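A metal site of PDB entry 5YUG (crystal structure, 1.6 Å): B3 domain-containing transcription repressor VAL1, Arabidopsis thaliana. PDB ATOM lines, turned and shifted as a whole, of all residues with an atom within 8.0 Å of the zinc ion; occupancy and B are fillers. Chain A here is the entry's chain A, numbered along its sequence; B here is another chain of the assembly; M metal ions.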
ATOM      1  N   TRP A  28      10.620  19.354  -1.256  1.00  0.00           N
ATOM      2  CA  TRP A  28      11.207  20.035  -0.112  1.00  0.00           C
ATOM      3  C   TRP A  28      12.538  19.389   0.296  1.00  0.00           C
ATOM      4  O   TRP A  28      12.809  18.229  -0.048  1.00  0.00           O
ATOM      5  CB  TRP A  28      10.215  19.986   1.052  1.00  0.00           C
ATOM      6  CG  TRP A  28       9.751  18.583   1.347  1.00  0.00           C
ATOM      7  CD1 TRP A  28      10.363  17.691   2.170  1.00  0.00           C
ATOM      8  CD2 TRP A  28       8.579  17.924   0.831  1.00  0.00           C
ATOM      9  NE1 TRP A  28       9.654  16.517   2.201  1.00  0.00           N
ATOM     10  CE2 TRP A  28       8.556  16.629   1.398  1.00  0.00           C
ATOM     11  CE3 TRP A  28       7.552  18.289  -0.054  1.00  0.00           C
ATOM     12  CZ2 TRP A  28       7.551  15.697   1.103  1.00  0.00           C
ATOM     13  CZ3 TRP A  28       6.539  17.354  -0.338  1.00  0.00           C
ATOM     14  CH2 TRP A  28       6.555  16.077   0.245  1.00  0.00           C
ATOM     15  N   PHE A  51       1.079  22.659  -2.616  1.00  0.00           N
ATOM     16  CA  PHE A  51       1.124  21.254  -2.229  1.00  0.00           C
ATOM     17  C   PHE A  51       0.183  20.959  -1.070  1.00  0.00           C
ATOM     18  O   PHE A  51      -0.610  20.001  -1.122  1.00  0.00           O
ATOM     19  CB  PHE A  51       2.573  20.851  -1.889  1.00  0.00           C
ATOM     20  CG  PHE A  51       2.731  19.377  -1.573  1.00  0.00           C
ATOM     21  CD1 PHE A  51       2.535  18.905  -0.285  1.00  0.00           C
ATOM     22  CD2 PHE A  51       3.093  18.462  -2.560  1.00  0.00           C
ATOM     23  CE1 PHE A  51       2.674  17.542   0.021  1.00  0.00           C
ATOM     24  CE2 PHE A  51       3.248  17.114  -2.264  1.00  0.00           C
ATOM     25  CZ  PHE A  51       3.017  16.655  -0.981  1.00  0.00           C
ATOM     26  N   CYS A  52       0.221  21.765  -0.004  1.00  0.00           N
ATOM     27  CA  CYS A  52      -0.594  21.419   1.145  1.00  0.00           C
ATOM     28  C   CYS A  52      -2.068  21.665   0.868  1.00  0.00           C
ATOM     29  O   CYS A  52      -2.915  20.951   1.407  1.00  0.00           O
ATOM     30  CB  CYS A  52      -0.119  22.177   2.380  1.00  0.00           C
ATOM     31  SG  CYS A  52       1.560  21.677   2.883  1.00  0.00           S
ATOM     32  N   GLU A  53      -2.387  22.660   0.023  1.00  0.00           N
ATOM     33  CA  GLU A  53      -3.776  22.836  -0.382  1.00  0.00           C
ATOM     34  C   GLU A  53      -4.294  21.637  -1.158  1.00  0.00           C
ATOM     35  O   GLU A  53      -5.443  21.211  -0.991  1.00  0.00           O
ATOM     36  CB  GLU A  53      -3.927  24.110  -1.240  1.00  0.00           C
ATOM     37  CG  GLU A  53      -3.826  25.420  -0.501  1.00  0.00           C
ATOM     38  CD  GLU A  53      -2.407  25.828  -0.179  1.00  0.00           C
ATOM     39  OE1 GLU A  53      -1.446  25.151  -0.602  1.00  0.00           O
ATOM     40  OE2 GLU A  53      -2.244  26.861   0.491  1.00  0.00           O
ATOM     41  N   PHE A  55      -3.089  18.461  -1.047  1.00  0.00           N
ATOM     42  CA  PHE A  55      -2.965  17.135  -0.443  1.00  0.00           C
ATOM     43  C   PHE A  55      -3.203  17.054   1.061  1.00  0.00           C
ATOM     44  O   PHE A  55      -3.416  15.948   1.566  1.00  0.00           O
ATOM     45  CB  PHE A  55      -1.575  16.546  -0.726  1.00  0.00           C
ATOM     46  CG  PHE A  55      -1.277  16.368  -2.186  1.00  0.00           C
ATOM     47  CD1 PHE A  55      -2.012  15.466  -2.941  1.00  0.00           C
ATOM     48  CD2 PHE A  55      -0.276  17.086  -2.817  1.00  0.00           C
ATOM     49  CE1 PHE A  55      -1.749  15.277  -4.276  1.00  0.00           C
ATOM     50  CE2 PHE A  55      -0.012  16.888  -4.163  1.00  0.00           C
ATOM     51  CZ  PHE A  55      -0.757  16.001  -4.885  1.00  0.00           C
ATOM     52  N   HIS A  56      -3.178  18.171   1.797  1.00  0.00           N
ATOM     53  CA  HIS A  56      -3.114  18.105   3.251  1.00  0.00           C
ATOM     54  C   HIS A  56      -4.300  18.773   3.947  1.00  0.00           C
ATOM     55  O   HIS A  56      -4.232  19.025   5.140  1.00  0.00           O
ATOM     56  CB  HIS A  56      -1.819  18.723   3.756  1.00  0.00           C
ATOM     57  CG  HIS A  56      -0.596  17.905   3.499  1.00  0.00           C
ATOM     58  ND1 HIS A  56       0.663  18.336   3.824  1.00  0.00           N
ATOM     59  CD2 HIS A  56      -0.442  16.665   2.963  1.00  0.00           C
ATOM     60  CE1 HIS A  56       1.555  17.403   3.513  1.00  0.00           C
ATOM     61  NE2 HIS A  56       0.897  16.383   2.982  1.00  0.00           N
ATOM     62  N   LYS A  57      -5.402  19.020   3.225  1.00  0.00           N
ATOM     63  CA  LYS A  57      -6.469  19.797   3.832  1.00  0.00           C
ATOM     64  C   LYS A  57      -7.128  19.092   5.014  1.00  0.00           C
ATOM     65  O   LYS A  57      -7.566  19.755   5.962  1.00  0.00           O
ATOM     66  CB  LYS A  57      -7.499  20.179   2.776  1.00  0.00           C
ATOM     67  CG  LYS A  57      -7.037  21.396   1.982  1.00  0.00           C
ATOM     68  CD  LYS A  57      -8.121  21.945   1.088  1.00  0.00           C
ATOM     69  CE  LYS A  57      -7.788  23.377   0.711  1.00  0.00           C
ATOM     70  NZ  LYS A  57      -8.916  24.078   0.036  1.00  0.00           N
ATOM     71  N   GLN A  59      -5.569  17.142   7.128  1.00  0.00           N
ATOM     72  CA  GLN A  59      -4.625  16.912   8.217  1.00  0.00           C
ATOM     73  C   GLN A  59      -4.773  17.972   9.296  1.00  0.00           C
ATOM     74  O   GLN A  59      -5.359  19.052   9.091  1.00  0.00           O
ATOM     75  CB  GLN A  59      -3.193  16.874   7.695  1.00  0.00           C
ATOM     76  CG  GLN A  59      -2.927  15.679   6.793  1.00  0.00           C
ATOM     77  CD  GLN A  59      -1.482  15.543   6.353  1.00  0.00           C
ATOM     78  OE1 GLN A  59      -0.605  16.273   6.802  1.00  0.00           O
ATOM     79  NE2 GLN A  59      -1.234  14.590   5.460  1.00  0.00           N
ATOM     80  N   SER A  60      -4.253  17.643  10.456  1.00  0.00           N
ATOM     81  CA  SER A  60      -4.127  18.602  11.541  1.00  0.00           C
ATOM     82  C   SER A  60      -3.000  19.595  11.237  1.00  0.00           C
ATOM     83  O   SER A  60      -2.177  19.401  10.331  1.00  0.00           O
ATOM     84  CB  SER A  60      -3.814  17.889  12.843  1.00  0.00           C
ATOM     85  OG  SER A  60      -2.646  17.096  12.706  1.00  0.00           O
ATOM     86  N   TRP A  62      -3.409  23.162  10.692  1.00  0.00           N
ATOM     87  CA  TRP A  62      -3.639  24.385   9.943  1.00  0.00           C
ATOM     88  C   TRP A  62      -3.886  25.561  10.872  1.00  0.00           C
ATOM     89  O   TRP A  62      -4.626  25.457  11.855  1.00  0.00           O
ATOM     90  CB  TRP A  62      -4.823  24.192   8.997  1.00  0.00           C
ATOM     91  CG  TRP A  62      -4.560  23.252   7.820  1.00  0.00           C
ATOM     92  CD1 TRP A  62      -4.765  21.904   7.791  1.00  0.00           C
ATOM     93  CD2 TRP A  62      -4.080  23.626   6.537  1.00  0.00           C
ATOM     94  NE1 TRP A  62      -4.445  21.400   6.536  1.00  0.00           N
ATOM     95  CE2 TRP A  62      -4.023  22.451   5.756  1.00  0.00           C
ATOM     96  CE3 TRP A  62      -3.696  24.843   5.956  1.00  0.00           C
ATOM     97  CZ2 TRP A  62      -3.602  22.464   4.424  1.00  0.00           C
ATOM     98  CZ3 TRP A  62      -3.285  24.862   4.647  1.00  0.00           C
ATOM     99  CH2 TRP A  62      -3.222  23.675   3.894  1.00  0.00           C
ATOM    100  N   LEU A  72      -2.418  28.184   6.562  1.00  0.00           N
ATOM    101  CA  LEU A  72      -1.018  27.798   6.524  1.00  0.00           C
ATOM    102  C   LEU A  72      -0.887  26.452   7.238  1.00  0.00           C
ATOM    103  O   LEU A  72      -1.267  26.331   8.415  1.00  0.00           O
ATOM    104  CB  LEU A  72      -0.168  28.869   7.215  1.00  0.00           C
ATOM    105  CG  LEU A  72      -0.197  30.295   6.655  1.00  0.00           C
ATOM    106  CD1 LEU A  72       0.602  31.226   7.575  1.00  0.00           C
ATOM    107  CD2 LEU A  72       0.427  30.333   5.257  1.00  0.00           C
ATOM    108  N   HIS A  73      -0.345  25.456   6.545  1.00  0.00           N
ATOM    109  CA  HIS A  73      -0.223  24.131   7.140  1.00  0.00           C
ATOM    110  C   HIS A  73       1.048  24.047   7.962  1.00  0.00           C
ATOM    111  O   HIS A  73       2.149  23.870   7.425  1.00  0.00           O
ATOM    112  CB  HIS A  73      -0.245  23.050   6.063  1.00  0.00           C
ATOM    113  CG  HIS A  73      -0.501  21.698   6.647  1.00  0.00           C
ATOM    114  ND1 HIS A  73      -0.058  20.531   6.076  1.00  0.00           N
ATOM    115  CD2 HIS A  73      -1.151  21.351   7.783  1.00  0.00           C
ATOM    116  CE1 HIS A  73      -0.428  19.514   6.842  1.00  0.00           C
ATOM    117  NE2 HIS A  73      -1.100  19.990   7.869  1.00  0.00           N
ATOM    118  N   CYS A  74       0.889  24.140   9.276  1.00  0.00           N
ATOM    119  CA  CYS A  74       2.019  24.125  10.203  1.00  0.00           C
ATOM    120  C   CYS A  74       2.396  22.686  10.594  1.00  0.00           C
ATOM    121  O   CYS A  74       1.642  21.734  10.364  1.00  0.00           O
ATOM    122  CB  CYS A  74       1.686  24.993  11.415  1.00  0.00           C
ATOM    123  SG  CYS A  74       1.241  26.714  11.045  1.00  0.00           S
ATOM    124  N   GLY A  75       3.580  22.544  11.180  1.00  0.00           N
ATOM    125  CA  GLY A  75       4.103  21.213  11.467  1.00  0.00           C
ATOM    126  C   GLY A  75       4.213  20.357  10.226  1.00  0.00           C
ATOM    127  O   GLY A  75       3.961  19.154  10.284  1.00  0.00           O
ATOM    128  N   CYS A  76       4.614  20.963   9.113  1.00  0.00           N
ATOM    129  CA  CYS A  76       4.626  20.273   7.836  1.00  0.00           C
ATOM    130  C   CYS A  76       5.814  20.736   7.020  1.00  0.00           C
ATOM    131  O   CYS A  76       5.900  21.903   6.628  1.00  0.00           O
ATOM    132  CB  CYS A  76       3.335  20.502   7.058  1.00  0.00           C
ATOM    133  SG  CYS A  76       3.365  19.666   5.455  1.00  0.00           S
ATOM    134  N   ILE A  77       6.721  19.795   6.726  1.00  0.00           N
ATOM    135  CA  ILE A  77       7.934  20.119   5.997  1.00  0.00           C
ATOM    136  C   ILE A  77       7.614  20.754   4.640  1.00  0.00           C
ATOM    137  O   ILE A  77       8.340  21.658   4.182  1.00  0.00           O
ATOM    138  CB  ILE A  77       8.784  18.826   5.878  1.00  0.00           C
ATOM    139  CG1 ILE A  77      10.215  19.120   5.441  1.00  0.00           C
ATOM    140  CG2 ILE A  77       8.097  17.819   4.957  1.00  0.00           C
ATOM    141  CD1 ILE A  77      11.140  17.941   5.674  1.00  0.00           C
ATOM    142  N   ALA A  78       6.498  20.358   4.015  1.00  0.00           N
ATOM    143  CA  ALA A  78       6.226  20.848   2.671  1.00  0.00           C
ATOM    144  C   ALA A  78       5.850  22.333   2.638  1.00  0.00           C
ATOM    145  O   ALA A  78       5.983  22.961   1.583  1.00  0.00           O
ATOM    146  CB  ALA A  78       5.120  20.023   2.013  1.00  0.00           C
ATOM    147  N   SER A  79       5.430  22.920   3.760  1.00  0.00           N
ATOM    148  CA  SER A  79       5.163  24.357   3.841  1.00  0.00           C
ATOM    149  C   SER A  79       6.178  25.098   4.697  1.00  0.00           C
ATOM    150  O   SER A  79       6.013  26.316   4.920  1.00  0.00           O
ATOM    151  CB  SER A  79       3.760  24.617   4.375  1.00  0.00           C
ATOM    152  OG  SER A  79       2.826  24.453   3.327  1.00  0.00           O
ATOM    153  N   LYS A  80       7.226  24.418   5.183  1.00  0.00           N
ATOM    154  CA  LYS A  80       8.156  25.103   6.077  1.00  0.00           C
ATOM    155  C   LYS A  80       8.636  26.419   5.470  1.00  0.00           C
ATOM    156  O   LYS A  80       8.753  27.438   6.166  1.00  0.00           O
ATOM    157  CB  LYS A  80       9.337  24.176   6.374  1.00  0.00           C
ATOM    158  CG  LYS A  80      10.339  24.720   7.400  1.00  0.00           C
ATOM    159  CD  LYS A  80      11.635  23.917   7.357  1.00  0.00           C
ATOM    160  CE  LYS A  80      12.589  24.359   8.463  1.00  0.00           C
ATOM    161  NZ  LYS A  80      13.538  23.275   8.832  1.00  0.00           N
ATOM    162  N   ILE A  83       6.145  29.794   5.955  1.00  0.00           N
ATOM    163  CA  ILE A  83       5.501  30.105   7.229  1.00  0.00           C
ATOM    164  C   ILE A  83       6.531  30.673   8.192  1.00  0.00           C
ATOM    165  O   ILE A  83       7.568  30.056   8.451  1.00  0.00           O
ATOM    166  CB  ILE A  83       4.853  28.842   7.843  1.00  0.00           C
ATOM    167  CG1 ILE A  83       3.753  28.326   6.923  1.00  0.00           C
ATOM    168  CG2 ILE A  83       4.346  29.122   9.238  1.00  0.00           C
ATOM    169  CD1 ILE A  83       3.314  26.925   7.256  1.00  0.00           C
ATOM    170  N   ARG B  63      -0.903  19.188  16.608  1.00  0.00           N
ATOM    171  CA  ARG B  63      -0.807  17.948  15.846  1.00  0.00           C
ATOM    172  C   ARG B  63      -0.406  16.838  16.793  1.00  0.00           C
ATOM    173  O   ARG B  63       0.026  17.091  17.917  1.00  0.00           O
ATOM    174  CB  ARG B  63       0.218  18.035  14.691  1.00  0.00           C
ATOM    175  CG  ARG B  63      -0.012  19.206  13.745  1.00  0.00           C
ATOM    176  CD  ARG B  63       0.711  18.970  12.425  1.00  0.00           C
ATOM    177  NE  ARG B  63       0.079  17.865  11.672  1.00  0.00           N
ATOM    178  CZ  ARG B  63       0.440  17.502  10.442  1.00  0.00           C
ATOM    179  NH1 ARG B  63       1.436  18.125   9.826  1.00  0.00           N
ATOM    180  NH2 ARG B  63      -0.191  16.506   9.839  1.00  0.00           N
ATOM    181  N   GLY B  89       6.160  14.357   6.063  1.00  0.00           N
ATOM    182  CA  GLY B  89       5.012  15.016   6.621  1.00  0.00           C
ATOM    183  C   GLY B  89       4.838  14.665   8.087  1.00  0.00           C
ATOM    184  O   GLY B  89       5.383  13.678   8.588  1.00  0.00           O
ATOM    185  N   GLY B  90       4.061  15.482   8.779  1.00  0.00           N
ATOM    186  CA  GLY B  90       3.825  15.267  10.192  1.00  0.00           C
ATOM    187  C   GLY B  90       5.012  15.688  11.032  1.00  0.00           C
ATOM    188  O   GLY B  90       6.008  16.254  10.563  1.00  0.00           O
HETATM  189 ZN    ZN M   1       1.353  20.149   4.560  1.00  0.00          ZN
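The backbone carbonyl oxygen (O) of His 56 lies within hydrogen-bond range of the indole nitrogen (NE1) of Trp 62 (2.8 Å).
A ring nitrogen (NE2) of His 73 sits at hydrogen-bond distance from the backbone carbonyl oxygen (O) of Ser 60.
SG of Cys 76 sits close to N of Ala 78, at 3.5 Å.
The side-chain hydroxyl of Ser 79 lies close to the side-chain sulfur of Cys 52, 3.1 Å away.
A ring nitrogen (ND1) of His 56 binds the zinc ion (2.1 Å).
ND1 of His 73 binds the zinc ion.
The zinc ion is bound by SG of Cys 76, 2.3 Å away.
The zinc ion is bound by SG of Cys 52 (2.3 Å).
Within 4 Å of the zinc ion: Cys 52, His 56, His 73 and Cys 76.
The nearest printed residue that does not touch the zinc ion is Ala 78 (4.5 Å).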
